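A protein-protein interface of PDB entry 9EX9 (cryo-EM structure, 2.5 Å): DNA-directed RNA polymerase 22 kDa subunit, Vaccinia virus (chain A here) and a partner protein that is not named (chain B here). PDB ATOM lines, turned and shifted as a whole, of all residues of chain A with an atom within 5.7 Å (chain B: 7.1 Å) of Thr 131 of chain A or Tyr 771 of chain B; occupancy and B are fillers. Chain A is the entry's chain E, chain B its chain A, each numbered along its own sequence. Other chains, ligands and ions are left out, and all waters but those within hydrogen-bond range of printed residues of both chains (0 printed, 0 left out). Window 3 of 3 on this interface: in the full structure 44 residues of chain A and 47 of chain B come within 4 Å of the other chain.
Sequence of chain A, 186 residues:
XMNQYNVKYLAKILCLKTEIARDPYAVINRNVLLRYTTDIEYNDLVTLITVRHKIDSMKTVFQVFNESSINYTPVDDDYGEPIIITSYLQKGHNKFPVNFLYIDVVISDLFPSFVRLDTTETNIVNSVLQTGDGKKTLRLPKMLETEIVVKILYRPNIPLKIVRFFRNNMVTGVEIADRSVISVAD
Among the printed residues, merely in contact across the chains: Val 128 of chain A with Gln 773 of chain B (3.7 Å), Thr 131 of chain A with Tyr 771 of chain B (3.5 Å) and Leu 138 of chain A with Asn 778 of chain B (3.6 Å).
Of the 17 printed residues of chain B, 3 touch a printed residue of chain A.
Hydrophobic or aromatic side chains of chain B within 4 Å of the printed part of chain A: Tyr 771.
Along chain B the printed residues that touch a printed residue of chain A span positions 771 to 778.
Among the printed residues, no Asp or Glu carboxylate lies within 4 Å of a Lys or Arg side-chain nitrogen of the other chain.
The backbone carbonyl oxygen (O) of Thr 137 of chain A is in hydrogen-bond range of the side-chain amide nitrogen (ND2) of Asn 778 of chain B (3.3 Å).
O of Leu 129 of chain A is in hydrogen-bond range of N of Leu 138 of chain A, 3.1 Å away.
OG1 of Thr 131 of chain A lies within hydrogen-bond range of O of Lys 136 of chain A, at 2.9 Å.
O of Tyr 771 of chain B lies within hydrogen-bond range of NZ of Lys 789 of chain B (3.0 Å).
OD1 of Asp 769 of chain B is in hydrogen-bond range of N of Gln 773 of chain B (2.8 Å).
The backbone NH (N) of Tyr 771 of chain B sits close to the side-chain carboxylate (OD1) of Asp 769 of chain B (3.2 Å).
Thr 131 of chain A touches one residue of chain B.
Of the printed residues of chain B, Leu 138 of chain A touches Asn 778 (3.6 Å).
Tyr 771 of chain B touches just one residue of chain A: Thr 131.
Printed residues of chain A within 4 Å of Gln 773 of chain B: Val 128 (3.7 Å).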
ATOM      1  N   VAL A 128      23.726  23.402 -10.619  1.00  0.00           N
ATOM      2  CA  VAL A 128      24.884  23.754 -11.428  1.00  0.00           C
ATOM      3  C   VAL A 128      25.549  22.514 -12.002  1.00  0.00           C
ATOM      4  O   VAL A 128      26.194  22.584 -13.053  1.00  0.00           O
ATOM      5  CB  VAL A 128      25.881  24.585 -10.605  1.00  0.00           C
ATOM      6  CG1 VAL A 128      27.200  24.701 -11.337  1.00  0.00           C
ATOM      7  CG2 VAL A 128      25.316  25.960 -10.329  1.00  0.00           C
ATOM      8  N   LEU A 129      25.425  21.367 -11.333  1.00  0.00           N
ATOM      9  CA  LEU A 129      26.127  20.178 -11.807  1.00  0.00           C
ATOM     10  C   LEU A 129      25.461  19.520 -13.009  1.00  0.00           C
ATOM     11  O   LEU A 129      26.130  18.775 -13.730  1.00  0.00           O
ATOM     12  CB  LEU A 129      26.257  19.158 -10.676  1.00  0.00           C
ATOM     13  CG  LEU A 129      27.354  19.445  -9.652  1.00  0.00           C
ATOM     14  CD1 LEU A 129      27.286  18.443  -8.525  1.00  0.00           C
ATOM     15  CD2 LEU A 129      28.725  19.419 -10.297  1.00  0.00           C
ATOM     16  N   GLN A 130      24.174  19.762 -13.246  1.00  0.00           N
ATOM     17  CA  GLN A 130      23.499  19.128 -14.371  1.00  0.00           C
ATOM     18  C   GLN A 130      24.066  19.624 -15.695  1.00  0.00           C
ATOM     19  O   GLN A 130      24.486  20.776 -15.825  1.00  0.00           O
ATOM     20  CB  GLN A 130      22.002  19.400 -14.320  1.00  0.00           C
ATOM     21  CG  GLN A 130      21.286  18.668 -13.219  1.00  0.00           C
ATOM     22  CD  GLN A 130      19.834  19.059 -13.121  1.00  0.00           C
ATOM     23  OE1 GLN A 130      19.280  19.661 -14.037  1.00  0.00           O
ATOM     24  NE2 GLN A 130      19.206  18.728 -12.004  1.00  0.00           N
ATOM     25  N   THR A 131      24.073  18.737 -16.687  1.00  0.00           N
ATOM     26  CA  THR A 131      24.629  19.046 -17.999  1.00  0.00           C
ATOM     27  C   THR A 131      23.616  19.659 -18.954  1.00  0.00           C
ATOM     28  O   THR A 131      23.994  20.053 -20.060  1.00  0.00           O
ATOM     29  CB  THR A 131      25.205  17.783 -18.641  1.00  0.00           C
ATOM     30  OG1 THR A 131      24.196  16.769 -18.687  1.00  0.00           O
ATOM     31  CG2 THR A 131      26.394  17.271 -17.851  1.00  0.00           C
ATOM     32  N   GLY A 132      22.346  19.741 -18.567  1.00  0.00           N
ATOM     33  CA  GLY A 132      21.331  20.323 -19.414  1.00  0.00           C
ATOM     34  C   GLY A 132      20.772  19.393 -20.465  1.00  0.00           C
ATOM     35  O   GLY A 132      19.854  19.793 -21.192  1.00  0.00           O
ATOM     36  N   ASP A 133      21.283  18.172 -20.566  1.00  0.00           N
ATOM     37  CA  ASP A 133      20.843  17.193 -21.555  1.00  0.00           C
ATOM     38  C   ASP A 133      20.092  16.091 -20.815  1.00  0.00           C
ATOM     39  O   ASP A 133      20.663  15.062 -20.454  1.00  0.00           O
ATOM     40  CB  ASP A 133      22.034  16.641 -22.332  1.00  0.00           C
ATOM     41  CG  ASP A 133      21.651  15.516 -23.267  1.00  0.00           C
ATOM     42  OD1 ASP A 133      20.818  15.743 -24.166  1.00  0.00           O
ATOM     43  OD2 ASP A 133      22.193  14.403 -23.106  1.00  0.00           O
ATOM     44  N   LYS A 135      18.734  14.372 -17.766  1.00  0.00           N
ATOM     45  CA  LYS A 135      19.055  14.344 -16.345  1.00  0.00           C
ATOM     46  C   LYS A 135      20.507  13.970 -16.082  1.00  0.00           C
ATOM     47  O   LYS A 135      20.883  13.779 -14.920  1.00  0.00           O
ATOM     48  CB  LYS A 135      18.126  13.375 -15.610  1.00  0.00           C
ATOM     49  CG  LYS A 135      16.698  13.872 -15.487  1.00  0.00           C
ATOM     50  CD  LYS A 135      15.850  12.918 -14.663  1.00  0.00           C
ATOM     51  CE  LYS A 135      14.434  13.441 -14.487  1.00  0.00           C
ATOM     52  NZ  LYS A 135      13.585  12.502 -13.704  1.00  0.00           N
ATOM     53  N   LYS A 136      21.333  13.865 -17.119  1.00  0.00           N
ATOM     54  CA  LYS A 136      22.742  13.569 -16.912  1.00  0.00           C
ATOM     55  C   LYS A 136      23.387  14.666 -16.076  1.00  0.00           C
ATOM     56  O   LYS A 136      23.065  15.849 -16.210  1.00  0.00           O
ATOM     57  CB  LYS A 136      23.459  13.438 -18.253  1.00  0.00           C
ATOM     58  CG  LYS A 136      22.895  12.353 -19.141  1.00  0.00           C
ATOM     59  CD  LYS A 136      23.673  12.245 -20.437  1.00  0.00           C
ATOM     60  CE  LYS A 136      23.109  11.152 -21.327  1.00  0.00           C
ATOM     61  NZ  LYS A 136      23.903  10.987 -22.574  1.00  0.00           N
ATOM     62  N   THR A 137      24.303  14.263 -15.200  1.00  0.00           N
ATOM     63  CA  THR A 137      24.900  15.192 -14.254  1.00  0.00           C
ATOM     64  C   THR A 137      26.352  14.813 -14.013  1.00  0.00           C
ATOM     65  O   THR A 137      26.758  13.668 -14.214  1.00  0.00           O
ATOM     66  CB  THR A 137      24.130  15.207 -12.931  1.00  0.00           C
ATOM     67  OG1 THR A 137      24.839  15.996 -11.972  1.00  0.00           O
ATOM     68  CG2 THR A 137      23.962  13.803 -12.394  1.00  0.00           C
ATOM     69  N   LEU A 138      27.131  15.800 -13.585  1.00  0.00           N
ATOM     70  CA  LEU A 138      28.513  15.586 -13.196  1.00  0.00           C
ATOM     71  C   LEU A 138      28.592  15.192 -11.725  1.00  0.00           C
ATOM     72  O   LEU A 138      27.599  15.202 -10.996  1.00  0.00           O
ATOM     73  CB  LEU A 138      29.344  16.841 -13.451  1.00  0.00           C
ATOM     74  CG  LEU A 138      29.435  17.338 -14.891  1.00  0.00           C
ATOM     75  CD1 LEU A 138      30.068  18.710 -14.923  1.00  0.00           C
ATOM     76  CD2 LEU A 138      30.227  16.378 -15.745  1.00  0.00           C
ATOM     77  N   VAL B 768      37.430  21.914 -21.325  1.00  0.00           N
ATOM     78  CA  VAL B 768      36.457  22.857 -20.790  1.00  0.00           C
ATOM     79  C   VAL B 768      35.097  22.508 -21.369  1.00  0.00           C
ATOM     80  O   VAL B 768      34.953  22.369 -22.588  1.00  0.00           O
ATOM     81  CB  VAL B 768      36.840  24.304 -21.129  1.00  0.00           C
ATOM     82  CG1 VAL B 768      35.819  25.261 -20.568  1.00  0.00           C
ATOM     83  CG2 VAL B 768      38.222  24.623 -20.598  1.00  0.00           C
ATOM     84  N   ASP B 769      34.100  22.356 -20.506  1.00  0.00           N
ATOM     85  CA  ASP B 769      32.765  21.999 -20.958  1.00  0.00           C
ATOM     86  C   ASP B 769      32.051  23.255 -21.449  1.00  0.00           C
ATOM     87  O   ASP B 769      32.655  24.316 -21.622  1.00  0.00           O
ATOM     88  CB  ASP B 769      31.998  21.292 -19.848  1.00  0.00           C
ATOM     89  CG  ASP B 769      31.551  22.229 -18.759  1.00  0.00           C
ATOM     90  OD1 ASP B 769      32.153  23.306 -18.619  1.00  0.00           O
ATOM     91  OD2 ASP B 769      30.601  21.884 -18.031  1.00  0.00           O
ATOM     92  N   GLY B 770      30.750  23.149 -21.681  1.00  0.00           N
ATOM     93  CA  GLY B 770      29.995  24.239 -22.257  1.00  0.00           C
ATOM     94  C   GLY B 770      29.649  25.362 -21.316  1.00  0.00           C
ATOM     95  O   GLY B 770      29.052  26.349 -21.751  1.00  0.00           O
ATOM     96  N   TYR B 771      29.994  25.244 -20.034  1.00  0.00           N
ATOM     97  CA  TYR B 771      29.710  26.271 -19.041  1.00  0.00           C
ATOM     98  C   TYR B 771      30.976  26.870 -18.447  1.00  0.00           C
ATOM     99  O   TYR B 771      30.924  27.463 -17.368  1.00  0.00           O
ATOM    100  CB  TYR B 771      28.843  25.703 -17.924  1.00  0.00           C
ATOM    101  CG  TYR B 771      27.529  25.134 -18.384  1.00  0.00           C
ATOM    102  CD1 TYR B 771      26.468  25.957 -18.703  1.00  0.00           C
ATOM    103  CD2 TYR B 771      27.344  23.768 -18.479  1.00  0.00           C
ATOM    104  CE1 TYR B 771      25.268  25.436 -19.117  1.00  0.00           C
ATOM    105  CE2 TYR B 771      26.147  23.241 -18.889  1.00  0.00           C
ATOM    106  CZ  TYR B 771      25.112  24.077 -19.202  1.00  0.00           C
ATOM    107  OH  TYR B 771      23.917  23.549 -19.610  1.00  0.00           O
ATOM    108  N   GLY B 772      32.111  26.729 -19.120  1.00  0.00           N
ATOM    109  CA  GLY B 772      33.346  27.293 -18.617  1.00  0.00           C
ATOM    110  C   GLY B 772      33.953  26.553 -17.452  1.00  0.00           C
ATOM    111  O   GLY B 772      34.721  27.145 -16.692  1.00  0.00           O
ATOM    112  N   GLN B 773      33.631  25.277 -17.288  1.00  0.00           N
ATOM    113  CA  GLN B 773      34.142  24.456 -16.205  1.00  0.00           C
ATOM    114  C   GLN B 773      35.166  23.474 -16.750  1.00  0.00           C
ATOM    115  O   GLN B 773      35.111  23.088 -17.917  1.00  0.00           O
ATOM    116  CB  GLN B 773      33.005  23.698 -15.523  1.00  0.00           C
ATOM    117  CG  GLN B 773      31.929  24.598 -14.971  1.00  0.00           C
ATOM    118  CD  GLN B 773      30.649  23.864 -14.686  1.00  0.00           C
ATOM    119  OE1 GLN B 773      30.453  22.742 -15.137  1.00  0.00           O
ATOM    120  NE2 GLN B 773      29.763  24.497 -13.936  1.00  0.00           N
ATOM    121  N   VAL B 774      36.107  23.079 -15.904  1.00  0.00           N
ATOM    122  CA  VAL B 774      37.124  22.102 -16.270  1.00  0.00           C
ATOM    123  C   VAL B 774      36.682  20.749 -15.733  1.00  0.00           C
ATOM    124  O   VAL B 774      36.538  20.576 -14.518  1.00  0.00           O
ATOM    125  CB  VAL B 774      38.503  22.488 -15.719  1.00  0.00           C
ATOM    126  CG1 VAL B 774      39.531  21.452 -16.113  1.00  0.00           C
ATOM    127  CG2 VAL B 774      38.909  23.845 -16.225  1.00  0.00           C
ATOM    128  N   ASN B 778      33.436  12.339 -16.425  1.00  0.00           N
ATOM    129  CA  ASN B 778      32.171  12.750 -15.831  1.00  0.00           C
ATOM    130  C   ASN B 778      32.377  13.417 -14.477  1.00  0.00           C
ATOM    131  O   ASN B 778      31.426  13.549 -13.702  1.00  0.00           O
ATOM    132  CB  ASN B 778      31.243  11.543 -15.697  1.00  0.00           C
ATOM    133  CG  ASN B 778      29.818  11.936 -15.409  1.00  0.00           C
ATOM    134  OD1 ASN B 778      29.112  12.438 -16.282  1.00  0.00           O
ATOM    135  ND2 ASN B 778      29.377  11.701 -14.184  1.00  0.00           N
ATOM    136  N   TYR B 783      35.581  24.744 -11.070  1.00  0.00           N
ATOM    137  CA  TYR B 783      34.395  25.519 -11.421  1.00  0.00           C
ATOM    138  C   TYR B 783      34.689  26.525 -12.523  1.00  0.00           C
ATOM    139  O   TYR B 783      33.971  26.591 -13.524  1.00  0.00           O
ATOM    140  CB  TYR B 783      33.866  26.244 -10.189  1.00  0.00           C
ATOM    141  CG  TYR B 783      32.977  25.427  -9.288  1.00  0.00           C
ATOM    142  CD1 TYR B 783      31.921  24.694  -9.796  1.00  0.00           C
ATOM    143  CD2 TYR B 783      33.188  25.406  -7.921  1.00  0.00           C
ATOM    144  CE1 TYR B 783      31.106  23.961  -8.968  1.00  0.00           C
ATOM    145  CE2 TYR B 783      32.382  24.674  -7.089  1.00  0.00           C
ATOM    146  CZ  TYR B 783      31.344  23.954  -7.615  1.00  0.00           C
ATOM    147  OH  TYR B 783      30.542  23.225  -6.779  1.00  0.00           O
ATOM    148  N   ALA B 784      35.734  27.328 -12.355  1.00  0.00           N
ATOM    149  CA  ALA B 784      36.093  28.373 -13.302  1.00  0.00           C
ATOM    150  C   ALA B 784      37.409  28.013 -13.970  1.00  0.00           C
ATOM    151  O   ALA B 784      38.400  27.745 -13.285  1.00  0.00           O
ATOM    152  CB  ALA B 784      36.203  29.726 -12.601  1.00  0.00           C
ATOM    153  N   ALA B 785      37.425  28.037 -15.303  1.00  0.00           N
ATOM    154  CA  ALA B 785      38.556  27.489 -16.045  1.00  0.00           C
ATOM    155  C   ALA B 785      39.878  28.081 -15.575  1.00  0.00           C
ATOM    156  O   ALA B 785      40.704  27.383 -14.977  1.00  0.00           O
ATOM    157  CB  ALA B 785      38.364  27.730 -17.538  1.00  0.00           C
ATOM    158  N   LYS B 789      37.105  32.249 -16.370  1.00  0.00           N
ATOM    159  CA  LYS B 789      36.287  31.856 -17.519  1.00  0.00           C
ATOM    160  C   LYS B 789      36.599  32.728 -18.732  1.00  0.00           C
ATOM    161  O   LYS B 789      35.721  33.061 -19.529  1.00  0.00           O
ATOM    162  CB  LYS B 789      34.795  31.898 -17.186  1.00  0.00           C
ATOM    163  CG  LYS B 789      34.374  30.870 -16.162  1.00  0.00           C
ATOM    164  CD  LYS B 789      32.873  30.725 -16.094  1.00  0.00           C
ATOM    165  CE  LYS B 789      32.476  29.689 -15.070  1.00  0.00           C
ATOM    166  NZ  LYS B 789      31.022  29.425 -15.068  1.00  0.00           N
ATOM    167  N   TYR B 875      27.623  34.984 -14.795  1.00  0.00           N
ATOM    168  CA  TYR B 875      28.643  34.186 -15.461  1.00  0.00           C
ATOM    169  C   TYR B 875      29.318  33.166 -14.560  1.00  0.00           C
ATOM    170  O   TYR B 875      29.945  32.238 -15.077  1.00  0.00           O
ATOM    171  CB  TYR B 875      29.719  35.098 -16.061  1.00  0.00           C
ATOM    172  CG  TYR B 875      29.254  35.847 -17.284  1.00  0.00           C
ATOM    173  CD1 TYR B 875      28.544  37.028 -17.171  1.00  0.00           C
ATOM    174  CD2 TYR B 875      29.527  35.368 -18.553  1.00  0.00           C
ATOM    175  CE1 TYR B 875      28.118  37.709 -18.285  1.00  0.00           C
ATOM    176  CE2 TYR B 875      29.107  36.041 -19.669  1.00  0.00           C
ATOM    177  CZ  TYR B 875      28.403  37.210 -19.531  1.00  0.00           C
ATOM    178  OH  TYR B 875      27.982  37.883 -20.649  1.00  0.00           O
ATOM    179  N   PHE B 877      27.432  32.008 -11.689  1.00  0.00           N
ATOM    180  CA  PHE B 877      26.308  31.252 -11.145  1.00  0.00           C
ATOM    181  C   PHE B 877      26.311  31.233  -9.620  1.00  0.00           C
ATOM    182  O   PHE B 877      25.794  30.302  -9.004  1.00  0.00           O
ATOM    183  CB  PHE B 877      26.297  29.825 -11.695  1.00  0.00           C
ATOM    184  CG  PHE B 877      26.453  29.750 -13.187  1.00  0.00           C
ATOM    185  CD1 PHE B 877      25.825  30.657 -14.011  1.00  0.00           C
ATOM    186  CD2 PHE B 877      27.240  28.776 -13.765  1.00  0.00           C
ATOM    187  CE1 PHE B 877      25.976  30.590 -15.373  1.00  0.00           C
ATOM    188  CE2 PHE B 877      27.391  28.713 -15.129  1.00  0.00           C
ATOM    189  CZ  PHE B 877      26.759  29.619 -15.928  1.00  0.00           C
ATOM    190  N   LEU B 920      36.508  32.391 -24.453  1.00  0.00           N
ATOM    191  CA  LEU B 920      36.656  30.985 -24.096  1.00  0.00           C
ATOM    192  C   LEU B 920      35.415  30.211 -24.514  1.00  0.00           C
ATOM    193  O   LEU B 920      34.291  30.649 -24.255  1.00  0.00           O
ATOM    194  CB  LEU B 920      36.886  30.832 -22.594  1.00  0.00           C
ATOM    195  CG  LEU B 920      37.275  29.437 -22.104  1.00  0.00           C
ATOM    196  CD1 LEU B 920      38.674  29.084 -22.545  1.00  0.00           C
ATOM    197  CD2 LEU B 920      37.165  29.353 -20.603  1.00  0.00           C
ATOM    198  N   GLY B 922      33.619  26.047 -25.274  1.00  0.00           N
ATOM    199  CA  GLY B 922      33.663  24.645 -24.909  1.00  0.00           C
ATOM    200  C   GLY B 922      34.492  23.826 -25.876  1.00  0.00           C
ATOM    201  O   GLY B 922      34.561  24.104 -27.071  1.00  0.00           O
ATOM    202  N   TYR B1251      33.959  18.734 -30.503  1.00  0.00           N
ATOM    203  CA  TYR B1251      33.259  18.688 -29.230  1.00  0.00           C
ATOM    204  C   TYR B1251      31.747  18.771 -29.387  1.00  0.00           C
ATOM    205  O   TYR B1251      31.029  18.490 -28.423  1.00  0.00           O
ATOM    206  CB  TYR B1251      33.756  19.822 -28.337  1.00  0.00           C
ATOM    207  CG  TYR B1251      33.172  19.808 -26.953  1.00  0.00           C
ATOM    208  CD1 TYR B1251      33.618  18.907 -26.003  1.00  0.00           C
ATOM    209  CD2 TYR B1251      32.180  20.698 -26.590  1.00  0.00           C
ATOM    210  CE1 TYR B1251      33.089  18.889 -24.738  1.00  0.00           C
ATOM    211  CE2 TYR B1251      31.645  20.686 -25.330  1.00  0.00           C
ATOM    212  CZ  TYR B1251      32.104  19.779 -24.408  1.00  0.00           C
ATOM    213  OH  TYR B1251      31.573  19.763 -23.143  1.00  0.00           O
